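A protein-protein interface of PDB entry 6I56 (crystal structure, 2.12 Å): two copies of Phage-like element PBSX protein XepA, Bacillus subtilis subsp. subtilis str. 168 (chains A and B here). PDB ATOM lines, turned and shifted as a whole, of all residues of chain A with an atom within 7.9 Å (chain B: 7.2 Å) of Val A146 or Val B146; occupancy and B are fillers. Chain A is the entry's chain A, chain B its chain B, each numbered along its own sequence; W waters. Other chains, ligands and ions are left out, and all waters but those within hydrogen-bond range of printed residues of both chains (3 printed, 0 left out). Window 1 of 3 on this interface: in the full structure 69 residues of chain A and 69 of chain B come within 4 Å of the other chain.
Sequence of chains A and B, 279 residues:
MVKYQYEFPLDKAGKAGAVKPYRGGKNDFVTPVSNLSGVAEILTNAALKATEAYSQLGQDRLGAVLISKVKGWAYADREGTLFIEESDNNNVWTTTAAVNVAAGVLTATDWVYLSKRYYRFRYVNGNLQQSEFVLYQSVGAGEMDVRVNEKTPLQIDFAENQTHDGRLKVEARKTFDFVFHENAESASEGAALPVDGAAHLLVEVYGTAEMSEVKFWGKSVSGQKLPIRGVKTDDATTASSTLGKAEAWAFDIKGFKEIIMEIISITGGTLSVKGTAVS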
ATOM      1  N   GLU A 143       2.479   0.657   2.392  1.00  0.00           N
ATOM      2  CA  GLU A 143       2.441  -0.765   2.010  1.00  0.00           C
ATOM      3  C   GLU A 143       1.492  -1.469   2.976  1.00  0.00           C
ATOM      4  O   GLU A 143       1.767  -1.478   4.175  1.00  0.00           O
ATOM      5  CB  GLU A 143       3.849  -1.342   1.986  1.00  0.00           C
ATOM      6  CG  GLU A 143       3.899  -2.730   1.368  1.00  0.00           C
ATOM      7  CD  GLU A 143       5.282  -3.318   1.229  1.00  0.00           C
ATOM      8  OE1 GLU A 143       5.982  -3.456   2.225  1.00  0.00           O
ATOM      9  OE2 GLU A 143       5.643  -3.623   0.127  1.00  0.00           O
ATOM     10  N   MET A 144       0.420  -2.023   2.427  1.00  0.00           N
ATOM     11  CA  MET A 144      -0.669  -2.740   3.111  1.00  0.00           C
ATOM     12  C   MET A 144      -0.326  -4.246   3.147  1.00  0.00           C
ATOM     13  O   MET A 144      -0.001  -4.817   2.062  1.00  0.00           O
ATOM     14  CB  MET A 144      -1.991  -2.505   2.363  1.00  0.00           C
ATOM     15  CG  MET A 144      -3.227  -2.945   3.124  1.00  0.00           C
ATOM     16  SD  MET A 144      -3.253  -2.471   4.936  1.00  0.00           S
ATOM     17  CE  MET A 144      -4.320  -3.698   5.706  1.00  0.00           C
ATOM     18  N   ASP A 145      -0.392  -4.864   4.319  1.00  0.00           N
ATOM     19  CA  ASP A 145      -0.339  -6.333   4.414  1.00  0.00           C
ATOM     20  C   ASP A 145      -1.686  -6.910   3.939  1.00  0.00           C
ATOM     21  O   ASP A 145      -2.748  -6.375   4.299  1.00  0.00           O
ATOM     22  CB  ASP A 145       0.040  -6.767   5.829  1.00  0.00           C
ATOM     23  CG  ASP A 145       1.454  -6.369   6.153  1.00  0.00           C
ATOM     24  OD1 ASP A 145       2.369  -6.986   5.604  1.00  0.00           O
ATOM     25  OD2 ASP A 145       1.611  -5.378   6.917  1.00  0.00           O
ATOM     26  N   VAL A 146      -1.622  -7.944   3.143  1.00  0.00           N
ATOM     27  CA  VAL A 146      -2.806  -8.638   2.578  1.00  0.00           C
ATOM     28  C   VAL A 146      -2.623 -10.154   2.716  1.00  0.00           C
ATOM     29  O   VAL A 146      -1.492 -10.672   2.686  1.00  0.00           O
ATOM     30  CB  VAL A 146      -3.084  -8.236   1.106  1.00  0.00           C
ATOM     31  CG1 VAL A 146      -3.305  -6.738   0.976  1.00  0.00           C
ATOM     32  CG2 VAL A 146      -1.983  -8.674   0.169  1.00  0.00           C
ATOM     33  N   ARG A 147      -3.749 -10.830   2.815  1.00  0.00           N
ATOM     34  CA  ARG A 147      -3.837 -12.308   2.761  1.00  0.00           C
ATOM     35  C   ARG A 147      -4.614 -12.662   1.493  1.00  0.00           C
ATOM     36  O   ARG A 147      -5.770 -12.226   1.346  1.00  0.00           O
ATOM     37  CB  ARG A 147      -4.523 -12.833   4.008  1.00  0.00           C
ATOM     38  CG  ARG A 147      -4.629 -14.348   4.047  1.00  0.00           C
ATOM     39  CD  ARG A 147      -3.437 -14.989   4.681  1.00  0.00           C
ATOM     40  NE  ARG A 147      -3.236 -14.471   6.037  1.00  0.00           N
ATOM     41  CZ  ARG A 147      -3.329 -15.166   7.146  1.00  0.00           C
ATOM     42  NH1 ARG A 147      -3.637 -16.433   7.094  1.00  0.00           N
ATOM     43  NH2 ARG A 147      -3.158 -14.574   8.313  1.00  0.00           N
ATOM     44  N   VAL A 148      -3.957 -13.372   0.598  1.00  0.00           N
ATOM     45  CA  VAL A 148      -4.544 -13.794  -0.692  1.00  0.00           C
ATOM     46  C   VAL A 148      -5.334 -15.076  -0.442  1.00  0.00           C
ATOM     47  O   VAL A 148      -4.786 -16.002   0.108  1.00  0.00           O
ATOM     48  CB  VAL A 148      -3.476 -13.955  -1.768  1.00  0.00           C
ATOM     49  CG1 VAL A 148      -4.082 -14.501  -3.053  1.00  0.00           C
ATOM     50  CG2 VAL A 148      -2.733 -12.669  -2.020  1.00  0.00           C
ATOM     51  N   ASN A 149      -6.630 -15.041  -0.676  1.00  0.00           N
ATOM     52  CA  ASN A 149      -7.584 -16.160  -0.553  1.00  0.00           C
ATOM     53  C   ASN A 149      -7.955 -16.500  -1.985  1.00  0.00           C
ATOM     54  O   ASN A 149      -8.456 -15.599  -2.671  1.00  0.00           O
ATOM     55  CB  ASN A 149      -8.780 -15.766   0.311  1.00  0.00           C
ATOM     56  CG  ASN A 149      -8.311 -15.254   1.674  1.00  0.00           C
ATOM     57  OD1 ASN A 149      -7.721 -16.014   2.451  1.00  0.00           O
ATOM     58  ND2 ASN A 149      -8.504 -13.978   1.989  1.00  0.00           N
ATOM     59  N   GLU A 150      -7.609 -17.679  -2.483  1.00  0.00           N
ATOM     60  CA  GLU A 150      -7.995 -18.078  -3.871  1.00  0.00           C
ATOM     61  C   GLU A 150      -8.932 -19.301  -3.791  1.00  0.00           C
ATOM     62  O   GLU A 150      -8.701 -20.224  -2.989  1.00  0.00           O
ATOM     63  CB  GLU A 150      -6.755 -18.272  -4.756  1.00  0.00           C
ATOM     64  CG  GLU A 150      -6.166 -19.667  -4.591  1.00  0.00           C
ATOM     65  CD  GLU A 150      -4.792 -19.932  -5.172  1.00  0.00           C
ATOM     66  OE1 GLU A 150      -4.288 -19.123  -6.003  1.00  0.00           O
ATOM     67  OE2 GLU A 150      -4.226 -20.958  -4.784  1.00  0.00           O
ATOM     68  N   GLY B 142      -2.560  -4.426  10.885  1.00  0.00           N
ATOM     69  CA  GLY B 142      -3.649  -5.201  10.281  1.00  0.00           C
ATOM     70  C   GLY B 142      -3.244  -5.858   8.975  1.00  0.00           C
ATOM     71  O   GLY B 142      -2.038  -5.804   8.577  1.00  0.00           O
ATOM     72  N   GLU B 143      -4.206  -6.492   8.340  1.00  0.00           N
ATOM     73  CA  GLU B 143      -4.036  -7.362   7.159  1.00  0.00           C
ATOM     74  C   GLU B 143      -5.423  -7.504   6.527  1.00  0.00           C
ATOM     75  O   GLU B 143      -6.371  -8.001   7.187  1.00  0.00           O
ATOM     76  CB  GLU B 143      -3.417  -8.675   7.615  1.00  0.00           C
ATOM     77  CG  GLU B 143      -3.165  -9.704   6.518  1.00  0.00           C
ATOM     78  CD  GLU B 143      -2.456 -10.975   6.997  1.00  0.00           C
ATOM     79  OE1 GLU B 143      -3.065 -12.028   7.006  1.00  0.00           O
ATOM     80  OE2 GLU B 143      -1.283 -10.908   7.284  1.00  0.00           O
ATOM     81  N   MET B 144      -5.502  -7.112   5.258  1.00  0.00           N
ATOM     82  CA  MET B 144      -6.706  -7.111   4.398  1.00  0.00           C
ATOM     83  C   MET B 144      -6.805  -8.450   3.656  1.00  0.00           C
ATOM     84  O   MET B 144      -5.778  -8.896   3.069  1.00  0.00           O
ATOM     85  CB  MET B 144      -6.512  -5.992   3.381  1.00  0.00           C
ATOM     86  CG  MET B 144      -7.697  -5.583   2.576  1.00  0.00           C
ATOM     87  SD  MET B 144      -7.008  -4.068   1.785  1.00  0.00           S
ATOM     88  CE  MET B 144      -7.037  -2.849   3.097  1.00  0.00           C
ATOM     89  N   ASP B 145      -7.951  -9.128   3.715  1.00  0.00           N
ATOM     90  CA  ASP B 145      -8.183 -10.298   2.839  1.00  0.00           C
ATOM     91  C   ASP B 145      -8.443  -9.776   1.420  1.00  0.00           C
ATOM     92  O   ASP B 145      -9.186  -8.772   1.276  1.00  0.00           O
ATOM     93  CB  ASP B 145      -9.272 -11.164   3.423  1.00  0.00           C
ATOM     94  CG  ASP B 145      -8.855 -11.806   4.732  1.00  0.00           C
ATOM     95  OD1 ASP B 145      -8.146 -12.766   4.684  1.00  0.00           O
ATOM     96  OD2 ASP B 145      -9.297 -11.332   5.786  1.00  0.00           O
ATOM     97  N   VAL B 146      -7.797 -10.384   0.424  1.00  0.00           N
ATOM     98  CA  VAL B 146      -7.951  -9.999  -1.011  1.00  0.00           C
ATOM     99  C   VAL B 146      -8.121 -11.276  -1.840  1.00  0.00           C
ATOM    100  O   VAL B 146      -7.626 -12.345  -1.455  1.00  0.00           O
ATOM    101  CB  VAL B 146      -6.777  -9.140  -1.534  1.00  0.00           C
ATOM    102  CG1 VAL B 146      -6.549  -7.907  -0.676  1.00  0.00           C
ATOM    103  CG2 VAL B 146      -5.472  -9.885  -1.633  1.00  0.00           C
ATOM    104  N   ARG B 147      -8.822 -11.165  -2.947  1.00  0.00           N
ATOM    105  CA  ARG B 147      -9.004 -12.209  -3.968  1.00  0.00           C
ATOM    106  C   ARG B 147      -8.376 -11.681  -5.247  1.00  0.00           C
ATOM    107  O   ARG B 147      -8.741 -10.580  -5.727  1.00  0.00           O
ATOM    108  CB  ARG B 147     -10.496 -12.486  -4.140  1.00  0.00           C
ATOM    109  CG  ARG B 147     -10.856 -13.475  -5.244  1.00  0.00           C
ATOM    110  CD  ARG B 147     -10.860 -14.871  -4.734  1.00  0.00           C
ATOM    111  NE  ARG B 147     -11.789 -15.038  -3.614  1.00  0.00           N
ATOM    112  CZ  ARG B 147     -12.884 -15.771  -3.640  1.00  0.00           C
ATOM    113  NH1 ARG B 147     -13.216 -16.420  -4.752  1.00  0.00           N
ATOM    114  NH2 ARG B 147     -13.632 -15.883  -2.546  1.00  0.00           N
ATOM    115  N   VAL B 148      -7.405 -12.407  -5.751  1.00  0.00           N
ATOM    116  CA  VAL B 148      -6.699 -12.035  -7.005  1.00  0.00           C
ATOM    117  C   VAL B 148      -7.548 -12.524  -8.172  1.00  0.00           C
ATOM    118  O   VAL B 148      -8.016 -13.730  -8.139  1.00  0.00           O
ATOM    119  CB  VAL B 148      -5.296 -12.623  -7.072  1.00  0.00           C
ATOM    120  CG1 VAL B 148      -4.694 -12.311  -8.453  1.00  0.00           C
ATOM    121  CG2 VAL B 148      -4.439 -12.097  -5.921  1.00  0.00           C
HETATM  122  O   HOH W   1      -0.730  -3.631   6.903  1.00  0.00           O
HETATM  123  O   HOH W   2       0.363  -5.436   9.318  1.00  0.00           O
HETATM  124  O   HOH W   3      -6.978 -15.126  -4.877  1.00  0.00           O
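O of Arg A147 lies within hydrogen-bond range of ND2 of Asn A149 (3.3 Å).
Val A146 touches Met B144, but with the chains exchanged Met A144 does not touch Val B146 (7.1 Å).
Arg A147 touches Glu B143, but with the chains exchanged Glu A143 does not touch Arg B147 (15.3 Å).
Arg A147 touches Met B144, but with the chains exchanged Met A144 does not touch Arg B147 (11.7 Å).
Val A148 touches Val B146, but with the chains exchanged Val A146 does not touch Val B148 (7.4 Å).
Positions printed for both chains: 143, 144, 145, 146, 147 and 148.
Printed residues of chain A that touch a printed residue of chain B: Met A144, Asp A145, Val A146, Arg A147, Val A148 and Asn A149.
Hydrophobic or aromatic side chains of chain B that line the printed part of chain A: Met B144, Val B146 and Val B148.
Water W2 bridges O of Gly B142 (2.5 Å) and OD2 of Asp A145 (2.7 Å).
Water W3 bridges the backbone carbonyl oxygen (O) of Asn A149 and the backbone NH (N) of Val B148.
Water W1 lies within hydrogen-bond range of the backbone NH of Asp A145 (2.9 Å), the backbone carbonyl oxygen of Gly B142 (3.0 Å) and the side-chain sulfur of Met A144 (3.4 Å).
The backbone carbonyl oxygen of Asp A145 lies within hydrogen-bond range of the backbone NH of Met B144 (3.0 Å).
NE of Arg A147 lies within salt-bridge range of OE1 of Glu B143 (2.6 Å).
O of Met B144 is in hydrogen-bond range of N of Arg A147 (2.8 Å).
O of Arg A147 lies within hydrogen-bond range of N of Val B146.
The side-chain amide nitrogen (ND2) of Asn A149 lies within hydrogen-bond range of the side-chain carboxylate (OD1) of Asp B145 (3.0 Å).
The backbone NH (N) of Asn A149 sits at hydrogen-bond distance from the backbone carbonyl oxygen (O) of Val B146, 3.0 Å away.
Met A144 touches Glu B143.
Met B144 touches Met A144.
Gly B142 touches Asp A145 (O to CB, 3.6 Å).
Asp A145 touches Glu B143.
Glu B143 touches Val A146 (CG to C, 3.9 Å).
Val A146 touches Met B144.
Arg A147 touches Asp B145 (O to CA, 3.4 Å).
O of Val B146 touches CA of Val A148, at 3.5 Å.
CG1 of Val A148 touches CG2 of Val B148, at 3.8 Å.
O of Asn A149 touches CD of Arg B147, at 3.3 Å.
Printed residues of chain B within 4 Å of Met A144: Glu B143 (3.8 Å) and Met B144 (3.6 Å).
Of the printed residues of chain B, Val A146 touches Glu B143, Met B144 and Val B146.
Printed residues of chain A within 4 Å of Gly B142: Asp A145 (3.6 Å).
Printed residues of chain A within 4 Å of Glu B143: Met A144 (3.8 Å), Asp A145 (3.3 Å), Val A146 (3.9 Å) and Arg A147 (2.6 Å).
Of the printed residues of chain A, Met B144 touches Met A144, Asp A145, Val A146 and Arg A147.
Of the printed residues of chain A, Asp B145 touches Arg A147 and Asn A149.
The nearest printed residue of chain B that does not touch Val A146 is Asp B145 (5.3 Å).
The nearest printed residue of chain A that does not touch Val B148 is Asn A149 (4.6 Å).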
